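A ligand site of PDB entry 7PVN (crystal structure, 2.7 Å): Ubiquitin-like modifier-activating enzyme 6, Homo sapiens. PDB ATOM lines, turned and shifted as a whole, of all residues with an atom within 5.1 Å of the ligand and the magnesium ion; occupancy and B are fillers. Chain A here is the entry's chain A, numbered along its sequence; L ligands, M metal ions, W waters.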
ATOM      1  N   ARG A  46      -2.104  -1.007  10.883  1.00  0.00           N
ATOM      2  CA  ARG A  46      -3.408  -1.028  11.533  1.00  0.00           C
ATOM      3  C   ARG A  46      -3.266  -1.066  13.056  1.00  0.00           C
ATOM      4  O   ARG A  46      -4.050  -0.437  13.797  1.00  0.00           O
ATOM      5  CB  ARG A  46      -4.219  -2.237  11.037  1.00  0.00           C
ATOM      6  CG  ARG A  46      -4.028  -2.652   9.551  1.00  0.00           C
ATOM      7  CD  ARG A  46      -4.018  -1.525   8.519  1.00  0.00           C
ATOM      8  NE  ARG A  46      -4.067  -2.055   7.156  1.00  0.00           N
ATOM      9  CZ  ARG A  46      -3.862  -1.345   6.044  1.00  0.00           C
ATOM     10  NH1 ARG A  46      -3.580  -0.066   6.099  1.00  0.00           N
ATOM     11  NH2 ARG A  46      -3.931  -1.936   4.858  1.00  0.00           N
ATOM     12  N   VAL A 466     -16.373 -17.469   3.475  1.00  0.00           N
ATOM     13  CA  VAL A 466     -16.342 -16.349   2.554  1.00  0.00           C
ATOM     14  C   VAL A 466     -15.390 -15.288   3.116  1.00  0.00           C
ATOM     15  O   VAL A 466     -15.659 -14.674   4.146  1.00  0.00           O
ATOM     16  CB  VAL A 466     -17.733 -15.770   2.300  1.00  0.00           C
ATOM     17  CG1 VAL A 466     -17.666 -14.769   1.181  1.00  0.00           C
ATOM     18  CG2 VAL A 466     -18.696 -16.901   1.958  1.00  0.00           C
ATOM     19  N   GLY A 467     -14.272 -15.097   2.432  1.00  0.00           N
ATOM     20  CA  GLY A 467     -13.231 -14.208   2.889  1.00  0.00           C
ATOM     21  C   GLY A 467     -12.141 -14.972   3.608  1.00  0.00           C
ATOM     22  O   GLY A 467     -12.435 -15.902   4.371  1.00  0.00           O
ATOM     23  N   CYS A 468     -10.880 -14.616   3.343  1.00  0.00           N
ATOM     24  CA  CYS A 468      -9.738 -15.259   3.994  1.00  0.00           C
ATOM     25  C   CYS A 468      -8.766 -14.185   4.497  1.00  0.00           C
ATOM     26  O   CYS A 468      -7.608 -14.114   4.089  1.00  0.00           O
ATOM     27  CB  CYS A 468      -9.059 -16.229   3.045  1.00  0.00           C
ATOM     28  SG  CYS A 468      -7.921 -17.357   3.865  1.00  0.00           S
ATOM     29  N   GLY A 469      -9.254 -13.362   5.412  1.00  0.00           N
ATOM     30  CA  GLY A 469      -8.491 -12.314   6.074  1.00  0.00           C
ATOM     31  C   GLY A 469      -8.008 -12.741   7.436  1.00  0.00           C
ATOM     32  O   GLY A 469      -7.587 -13.885   7.647  1.00  0.00           O
ATOM     33  N   ALA A 470      -8.041 -11.799   8.387  1.00  0.00           N
ATOM     34  CA  ALA A 470      -7.622 -12.109   9.747  1.00  0.00           C
ATOM     35  C   ALA A 470      -8.553 -13.135  10.387  1.00  0.00           C
ATOM     36  O   ALA A 470      -8.101 -14.194  10.853  1.00  0.00           O
ATOM     37  CB  ALA A 470      -7.593 -10.826  10.574  1.00  0.00           C
ATOM     38  N   THR A 496     -12.736 -18.961  -0.157  1.00  0.00           N
ATOM     39  CA  THR A 496     -12.673 -18.103  -1.334  1.00  0.00           C
ATOM     40  C   THR A 496     -12.237 -16.695  -0.963  1.00  0.00           C
ATOM     41  O   THR A 496     -12.753 -16.119   0.007  1.00  0.00           O
ATOM     42  CB  THR A 496     -14.022 -18.049  -2.067  1.00  0.00           C
ATOM     43  OG1 THR A 496     -13.880 -17.271  -3.267  1.00  0.00           O
ATOM     44  CG2 THR A 496     -15.118 -17.432  -1.187  1.00  0.00           C
ATOM     45  N   ASP A 497     -11.289 -16.145  -1.722  1.00  0.00           N
ATOM     46  CA  ASP A 497     -10.823 -14.772  -1.573  1.00  0.00           C
ATOM     47  C   ASP A 497     -10.217 -14.246  -2.869  1.00  0.00           C
ATOM     48  O   ASP A 497      -9.433 -14.959  -3.492  1.00  0.00           O
ATOM     49  CB  ASP A 497      -9.795 -14.659  -0.447  1.00  0.00           C
ATOM     50  CG  ASP A 497      -9.733 -13.239   0.143  1.00  0.00           C
ATOM     51  OD1 ASP A 497      -9.127 -12.362  -0.507  1.00  0.00           O
ATOM     52  OD2 ASP A 497     -10.303 -12.989   1.219  1.00  0.00           O
ATOM     53  N   PRO A 498     -10.534 -13.027  -3.284  1.00  0.00           N
ATOM     54  CA  PRO A 498      -9.932 -12.474  -4.495  1.00  0.00           C
ATOM     55  C   PRO A 498      -8.609 -11.743  -4.313  1.00  0.00           C
ATOM     56  O   PRO A 498      -7.954 -11.443  -5.319  1.00  0.00           O
ATOM     57  CB  PRO A 498     -11.013 -11.478  -4.968  1.00  0.00           C
ATOM     58  CG  PRO A 498     -11.561 -10.947  -3.695  1.00  0.00           C
ATOM     59  CD  PRO A 498     -11.593 -12.151  -2.742  1.00  0.00           C
ATOM     60  N   ASP A 499      -8.189 -11.485  -3.085  1.00  0.00           N
ATOM     61  CA  ASP A 499      -7.084 -10.577  -2.789  1.00  0.00           C
ATOM     62  C   ASP A 499      -5.778 -11.332  -2.552  1.00  0.00           C
ATOM     63  O   ASP A 499      -5.750 -12.532  -2.285  1.00  0.00           O
ATOM     64  CB  ASP A 499      -7.428  -9.728  -1.558  1.00  0.00           C
ATOM     65  CG  ASP A 499      -6.960  -8.306  -1.684  1.00  0.00           C
ATOM     66  OD1 ASP A 499      -5.823  -8.102  -2.185  1.00  0.00           O
ATOM     67  OD2 ASP A 499      -7.699  -7.392  -1.262  1.00  0.00           O
ATOM     68  N   SER A 504       1.185  -5.397   5.579  1.00  0.00           N
ATOM     69  CA  SER A 504       0.267  -4.983   6.643  1.00  0.00           C
ATOM     70  C   SER A 504      -0.588  -6.153   7.123  1.00  0.00           C
ATOM     71  O   SER A 504      -0.936  -6.220   8.311  1.00  0.00           O
ATOM     72  CB  SER A 504      -0.607  -3.843   6.136  1.00  0.00           C
ATOM     73  OG  SER A 504      -0.936  -4.008   4.768  1.00  0.00           O
ATOM     74  N   ASN A 505      -0.940  -7.070   6.225  1.00  0.00           N
ATOM     75  CA  ASN A 505      -1.720  -8.240   6.635  1.00  0.00           C
ATOM     76  C   ASN A 505      -0.944  -9.112   7.620  1.00  0.00           C
ATOM     77  O   ASN A 505      -1.546  -9.738   8.501  1.00  0.00           O
ATOM     78  CB  ASN A 505      -2.135  -9.052   5.409  1.00  0.00           C
ATOM     79  CG  ASN A 505      -2.895  -8.236   4.397  1.00  0.00           C
ATOM     80  OD1 ASN A 505      -3.365  -7.144   4.707  1.00  0.00           O
ATOM     81  ND2 ASN A 505      -3.036  -8.757   3.189  1.00  0.00           N
ATOM     82  N   ARG A 508      -1.621  -9.526  11.569  1.00  0.00           N
ATOM     83  CA  ARG A 508      -2.710 -10.281  12.187  1.00  0.00           C
ATOM     84  C   ARG A 508      -3.120 -11.557  11.452  1.00  0.00           C
ATOM     85  O   ARG A 508      -3.993 -12.287  11.964  1.00  0.00           O
ATOM     86  CB  ARG A 508      -3.926  -9.363  12.382  1.00  0.00           C
ATOM     87  CG  ARG A 508      -4.585  -8.860  11.121  1.00  0.00           C
ATOM     88  CD  ARG A 508      -5.531  -7.733  11.460  1.00  0.00           C
ATOM     89  NE  ARG A 508      -6.168  -7.184  10.265  1.00  0.00           N
ATOM     90  CZ  ARG A 508      -5.545  -6.425   9.380  1.00  0.00           C
ATOM     91  NH1 ARG A 508      -4.269  -6.133   9.522  1.00  0.00           N
ATOM     92  NH2 ARG A 508      -6.208  -5.970   8.333  1.00  0.00           N
ATOM     93  N   GLN A 509      -2.547 -11.871  10.291  1.00  0.00           N
ATOM     94  CA  GLN A 509      -2.821 -13.119   9.577  1.00  0.00           C
ATOM     95  C   GLN A 509      -1.619 -14.047   9.724  1.00  0.00           C
ATOM     96  O   GLN A 509      -0.652 -13.971   8.957  1.00  0.00           O
ATOM     97  CB  GLN A 509      -3.156 -12.832   8.104  1.00  0.00           C
ATOM     98  CG  GLN A 509      -4.581 -12.313   7.897  1.00  0.00           C
ATOM     99  CD  GLN A 509      -4.708 -11.284   6.780  1.00  0.00           C
ATOM    100  OE1 GLN A 509      -4.569 -11.604   5.602  1.00  0.00           O
ATOM    101  NE2 GLN A 509      -5.016 -10.048   7.146  1.00  0.00           N
ATOM    102  N   LYS A 521      -4.303 -15.161  -1.116  1.00  0.00           N
ATOM    103  CA  LYS A 521      -4.524 -15.466   0.293  1.00  0.00           C
ATOM    104  C   LYS A 521      -5.082 -16.873   0.468  1.00  0.00           C
ATOM    105  O   LYS A 521      -4.582 -17.646   1.294  1.00  0.00           O
ATOM    106  CB  LYS A 521      -5.490 -14.450   0.904  1.00  0.00           C
ATOM    107  CG  LYS A 521      -4.914 -13.084   1.138  1.00  0.00           C
ATOM    108  CD  LYS A 521      -6.023 -12.078   1.362  1.00  0.00           C
ATOM    109  CE  LYS A 521      -5.500 -10.817   2.015  1.00  0.00           C
ATOM    110  NZ  LYS A 521      -6.559  -9.777   2.092  1.00  0.00           N
ATOM    111  N   ASN A 543     -12.045 -16.416  -6.156  1.00  0.00           N
ATOM    112  CA  ASN A 543     -13.228 -15.722  -6.638  1.00  0.00           C
ATOM    113  C   ASN A 543     -13.841 -14.837  -5.564  1.00  0.00           C
ATOM    114  O   ASN A 543     -13.676 -15.035  -4.359  1.00  0.00           O
ATOM    115  CB  ASN A 543     -14.267 -16.723  -7.147  1.00  0.00           C
ATOM    116  CG  ASN A 543     -13.805 -17.423  -8.425  1.00  0.00           C
ATOM    117  OD1 ASN A 543     -13.233 -18.517  -8.388  1.00  0.00           O
ATOM    118  ND2 ASN A 543     -14.055 -16.774  -9.570  1.00  0.00           N
ATOM    119  N   LYS A 544     -14.581 -13.842  -6.034  1.00  0.00           N
ATOM    120  CA  LYS A 544     -15.294 -12.921  -5.159  1.00  0.00           C
ATOM    121  C   LYS A 544     -16.757 -13.322  -5.143  1.00  0.00           C
ATOM    122  O   LYS A 544     -17.334 -13.602  -6.201  1.00  0.00           O
ATOM    123  CB  LYS A 544     -15.132 -11.479  -5.649  1.00  0.00           C
ATOM    124  CG  LYS A 544     -15.623 -10.442  -4.666  1.00  0.00           C
ATOM    125  CD  LYS A 544     -15.522  -9.025  -5.224  1.00  0.00           C
ATOM    126  CE  LYS A 544     -16.789  -8.630  -5.959  1.00  0.00           C
ATOM    127  NZ  LYS A 544     -16.730  -7.240  -6.486  1.00  0.00           N
ATOM    128  N   VAL A 545     -17.342 -13.383  -3.958  1.00  0.00           N
ATOM    129  CA  VAL A 545     -18.709 -13.872  -3.820  1.00  0.00           C
ATOM    130  C   VAL A 545     -19.663 -12.720  -4.102  1.00  0.00           C
ATOM    131  O   VAL A 545     -20.038 -11.963  -3.198  1.00  0.00           O
ATOM    132  CB  VAL A 545     -18.935 -14.498  -2.441  1.00  0.00           C
ATOM    133  CG1 VAL A 545     -20.360 -14.999  -2.318  1.00  0.00           C
ATOM    134  CG2 VAL A 545     -17.951 -15.636  -2.234  1.00  0.00           C
ATOM    135  N   CYS A 546     -19.996 -12.547  -5.385  1.00  0.00           N
ATOM    136  CA  CYS A 546     -20.920 -11.546  -5.896  1.00  0.00           C
ATOM    137  C   CYS A 546     -21.827 -12.219  -6.918  1.00  0.00           C
ATOM    138  O   CYS A 546     -21.587 -13.374  -7.278  1.00  0.00           O
ATOM    139  CB  CYS A 546     -20.162 -10.377  -6.515  1.00  0.00           C
ATOM    140  SG  CYS A 546     -19.101 -10.840  -7.883  1.00  0.00           S
ATOM    141  N   ALA A 567     -16.146 -13.986   6.774  1.00  0.00           N
ATOM    142  CA  ALA A 567     -15.053 -13.176   7.299  1.00  0.00           C
ATOM    143  C   ALA A 567     -14.818 -11.982   6.374  1.00  0.00           C
ATOM    144  O   ALA A 567     -13.691 -11.747   5.928  1.00  0.00           O
ATOM    145  CB  ALA A 567     -13.785 -14.021   7.421  1.00  0.00           C
ATOM    146  N   LEU A 568     -15.872 -11.232   6.091  1.00  0.00           N
ATOM    147  CA  LEU A 568     -15.836 -10.177   5.085  1.00  0.00           C
ATOM    148  C   LEU A 568     -15.517  -8.832   5.737  1.00  0.00           C
ATOM    149  O   LEU A 568     -15.460  -8.709   6.968  1.00  0.00           O
ATOM    150  CB  LEU A 568     -17.176 -10.114   4.347  1.00  0.00           C
ATOM    151  CG  LEU A 568     -17.517 -11.335   3.504  1.00  0.00           C
ATOM    152  CD1 LEU A 568     -18.995 -11.382   3.223  1.00  0.00           C
ATOM    153  CD2 LEU A 568     -16.745 -11.349   2.202  1.00  0.00           C
ATOM    154  N   ASP A 569     -15.295  -7.813   4.906  1.00  0.00           N
ATOM    155  CA  ASP A 569     -15.088  -6.453   5.397  1.00  0.00           C
ATOM    156  C   ASP A 569     -16.143  -5.436   4.955  1.00  0.00           C
ATOM    157  O   ASP A 569     -16.022  -4.260   5.332  1.00  0.00           O
ATOM    158  CB  ASP A 569     -13.690  -5.937   5.003  1.00  0.00           C
ATOM    159  CG  ASP A 569     -13.440  -5.980   3.526  1.00  0.00           C
ATOM    160  OD1 ASP A 569     -14.360  -5.622   2.759  1.00  0.00           O
ATOM    161  OD2 ASP A 569     -12.305  -6.309   3.133  1.00  0.00           O
ATOM    162  N   ASN A 570     -17.143  -5.811   4.150  1.00  0.00           N
ATOM    163  CA  ASN A 570     -18.107  -4.848   3.635  1.00  0.00           C
ATOM    164  C   ASN A 570     -19.532  -5.374   3.792  1.00  0.00           C
ATOM    165  O   ASN A 570     -19.777  -6.558   3.597  1.00  0.00           O
ATOM    166  CB  ASN A 570     -17.842  -4.532   2.171  1.00  0.00           C
ATOM    167  CG  ASN A 570     -17.899  -5.767   1.291  1.00  0.00           C
ATOM    168  OD1 ASN A 570     -18.849  -5.962   0.540  1.00  0.00           O
ATOM    169  ND2 ASN A 570     -16.868  -6.609   1.386  1.00  0.00           N
ATOM    170  N   ALA A 573     -21.369  -7.349   0.689  1.00  0.00           N
ATOM    171  CA  ALA A 573     -21.108  -8.776   0.561  1.00  0.00           C
ATOM    172  C   ALA A 573     -21.858  -9.558   1.638  1.00  0.00           C
ATOM    173  O   ALA A 573     -22.387 -10.643   1.362  1.00  0.00           O
ATOM    174  CB  ALA A 573     -19.604  -9.035   0.676  1.00  0.00           C
ATOM    175  N   LYS A 851      -3.060   3.025  -1.008  1.00  0.00           N
ATOM    176  CA  LYS A 851      -2.696   3.706   0.226  1.00  0.00           C
ATOM    177  C   LYS A 851      -1.387   3.168   0.813  1.00  0.00           C
ATOM    178  O   LYS A 851      -0.630   3.929   1.422  1.00  0.00           O
ATOM    179  CB  LYS A 851      -3.826   3.591   1.243  1.00  0.00           C
ATOM    180  CG  LYS A 851      -4.123   2.176   1.753  1.00  0.00           C
ATOM    181  CD  LYS A 851      -5.609   1.956   2.003  1.00  0.00           C
ATOM    182  CE  LYS A 851      -5.905   0.529   2.453  1.00  0.00           C
ATOM    183  NZ  LYS A 851      -7.348   0.268   2.718  1.00  0.00           N
ATOM    184  N   ILE A 890      -9.127   2.876   6.102  1.00  0.00           N
ATOM    185  CA  ILE A 890      -8.449   1.834   6.856  1.00  0.00           C
ATOM    186  C   ILE A 890      -9.144   1.636   8.201  1.00  0.00           C
ATOM    187  O   ILE A 890      -9.513   2.612   8.877  1.00  0.00           O
ATOM    188  CB  ILE A 890      -6.973   2.200   7.064  1.00  0.00           C
ATOM    189  CG1 ILE A 890      -6.212   2.239   5.732  1.00  0.00           C
ATOM    190  CG2 ILE A 890      -6.315   1.230   8.025  1.00  0.00           C
ATOM    191  CD1 ILE A 890      -4.918   3.022   5.824  1.00  0.00           C
ATOM    192  N   ILE A 891      -9.328   0.391   8.589  1.00  0.00           N
ATOM    193  CA  ILE A 891      -9.954   0.032   9.854  1.00  0.00           C
ATOM    194  C   ILE A 891      -8.861  -0.405  10.831  1.00  0.00           C
ATOM    195  O   ILE A 891      -8.062  -1.285  10.488  1.00  0.00           O
ATOM    196  CB  ILE A 891     -10.984  -1.097   9.684  1.00  0.00           C
ATOM    197  CG1 ILE A 891     -12.004  -0.749   8.595  1.00  0.00           C
ATOM    198  CG2 ILE A 891     -11.721  -1.327  11.012  1.00  0.00           C
ATOM    199  CD1 ILE A 891     -12.755   0.541   8.808  1.00  0.00           C
HETATM  200  P1  LIG L   1      -6.931  -4.180   5.441  1.00  0.00           P
HETATM  201  O1  LIG L   1      -7.161  -3.428   6.734  1.00  0.00           O
HETATM  202  O2  LIG L   1      -5.544  -4.891   5.432  1.00  0.00           O
HETATM  203  O3  LIG L   1      -7.118  -3.315   4.154  1.00  0.00           O
HETATM  204  P2  LIG L   1      -7.919  -6.614   4.286  1.00  0.00           P
HETATM  205  O4  LIG L   1      -7.912  -6.200   2.856  1.00  0.00           O
HETATM  206  O5  LIG L   1      -6.762  -7.552   4.667  1.00  0.00           O
HETATM  207  O6  LIG L   1      -7.977  -5.351   5.246  1.00  0.00           O
HETATM  208  P3  LIG L   1      -9.581  -8.017   6.045  1.00  0.00           P
HETATM  209  O7  LIG L   1     -10.298  -7.074   6.931  1.00  0.00           O
HETATM  210  O8  LIG L   1      -8.234  -8.415   6.653  1.00  0.00           O
HETATM  211  O9  LIG L   1      -9.301  -7.309   4.658  1.00  0.00           O
HETATM  212  O10 LIG L   1     -10.421  -9.308   5.671  1.00  0.00           O
HETATM  213  C1  LIG L   1     -11.572  -9.233   4.807  1.00  0.00           C
HETATM  214  C2  LIG L   1     -11.347 -10.156   3.648  1.00  0.00           C
HETATM  215  O11 LIG L   1     -12.574 -10.289   2.893  1.00  0.00           O
HETATM  216  C3  LIG L   1     -10.265  -9.724   2.649  1.00  0.00           C
HETATM  217  O12 LIG L   1      -9.341 -10.782   2.407  1.00  0.00           O
HETATM  218  C4  LIG L   1     -11.049  -9.434   1.367  1.00  0.00           C
HETATM  219  O13 LIG L   1     -10.272  -9.794   0.233  1.00  0.00           O
HETATM  220  C5  LIG L   1     -12.223 -10.382   1.530  1.00  0.00           C
HETATM  221  N1  LIG L   1     -13.405 -10.105   0.740  1.00  0.00           N
HETATM  222  C6  LIG L   1     -14.170  -8.955   0.694  1.00  0.00           C
HETATM  223  N2  LIG L   1     -15.247  -9.071  -0.030  1.00  0.00           N
HETATM  224  C7  LIG L   1     -15.206 -10.367  -0.496  1.00  0.00           C
HETATM  225  C8  LIG L   1     -16.079 -11.131  -1.305  1.00  0.00           C
HETATM  226  N3  LIG L   1     -17.241 -10.670  -1.772  1.00  0.00           N
HETATM  227  N4  LIG L   1     -15.727 -12.402  -1.582  1.00  0.00           N
HETATM  228  C9  LIG L   1     -14.595 -12.886  -1.077  1.00  0.00           C
HETATM  229  N5  LIG L   1     -13.696 -12.265  -0.304  1.00  0.00           N
HETATM  230  C10 LIG L   1     -14.068 -11.014  -0.042  1.00  0.00           C
HETATM  231 MG    MG M   1     -10.701  -5.560   4.668  1.00  0.00          MG
HETATM  232 CA    CA M   2      -5.210  -6.449   0.483  1.00  0.00          CA
HETATM  233  O   HOH W   1      -6.502  -4.563   0.755  1.00  0.00           O
HETATM  234  O   HOH W   2     -10.686  -3.642   5.780  1.00  0.00           O
HETATM  235  O   HOH W   3     -10.386  -3.929   3.442  1.00  0.00           O
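Merely in contact with the ligand: Gly 467, Gly 469, Ala 470, Thr 496, Pro 498, Asp 499, Gln 509, Lys 544, Ala 567, Leu 568 and Ala 573.
Hydrophobic or aromatic side chains within 4 Å of the ligand: Pro 498, Val 545, Leu 568 and Ala 573.
Within 4 Å of the ligand: Arg 46, Gly 467, Gly 469, Ala 470, Thr 496, Asp 497, Pro 498, Asp 499, Asn 505, Arg 508, Gln 509, Lys 521, Lys 544, Val 545, Ala 567, Leu 568, Asp 569, Asn 570, Ala 573 and Lys 851.
Within 4 Å of the magnesium ion: Asp 569.
The magnesium ion is bound by water W3 (2.1 Å), water W2 (2.2 Å), an oxygen (O9) of the ligand (2.2 Å) and the side-chain carboxylate (OD2) of Asp 569 (2.3 Å).
Slightly farther from the magnesium ion lies O7 of the ligand (2.8 Å).
Slightly farther from the magnesium ion lies O6 of the ligand (2.8 Å).
The side-chain carboxylate (OD1) of Asp 569 sits at hydrogen-bond distance from the side-chain amide nitrogen (ND2) of Asn 570.
OD1 of Asp 497 lies within hydrogen-bond range of N of Asp 499, at 2.9 Å.
N of Lys 521 lies within hydrogen-bond range of O of Asp 499 (3.2 Å).
OD1 of Asn 570 is in hydrogen-bond range of N of Ala 573, 2.9 Å away.
The side-chain sulfur (SG) of Cys 546 sits at hydrogen-bond distance from the backbone carbonyl oxygen (O) of Lys 544, at 3.7 Å.
The backbone NH of Ala 567 lies within hydrogen-bond range of the backbone carbonyl oxygen of Val 466 (2.8 Å).
The backbone carbonyl oxygen (O) of Thr 496 sits at hydrogen-bond distance from the backbone NH (N) of Gly 467 (3.0 Å).
The backbone carbonyl oxygen (O) of Asn 543 is in hydrogen-bond range of the side-chain hydroxyl (OG1) of Thr 496.
OD2 of Asp 497 lies within hydrogen-bond range of O12 of the ligand, 2.7 Å away.
An oxygen (O5) of the ligand is in salt-bridge range of the side-chain amino group (NZ) of Lys 521, at 3.4 Å.
N of Val 545 lies within hydrogen-bond range of N4 of the ligand, 3.0 Å away.
The backbone carbonyl oxygen (O) of Val 545 sits at hydrogen-bond distance from a nitrogen (N3) of the ligand (3.4 Å).
An oxygen (O1) of the ligand is in salt-bridge range of the guanidinium group (NH2) of Arg 508, at 3.2 Å.
The side-chain amide oxygen (OD1) of Asn 505 sits close to an oxygen (O2) of the ligand (3.2 Å).
The side-chain amide nitrogen of Asn 570 is in hydrogen-bond range of a nitrogen (N2) of the ligand (3.3 Å).
The guanidinium group (NE) of Arg 46 lies within salt-bridge range of an oxygen (O1) of the ligand, 3.4 Å away.
The side-chain amino group (NZ) of Lys 851 is in salt-bridge range of an oxygen (O3) of the ligand (3.9 Å).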
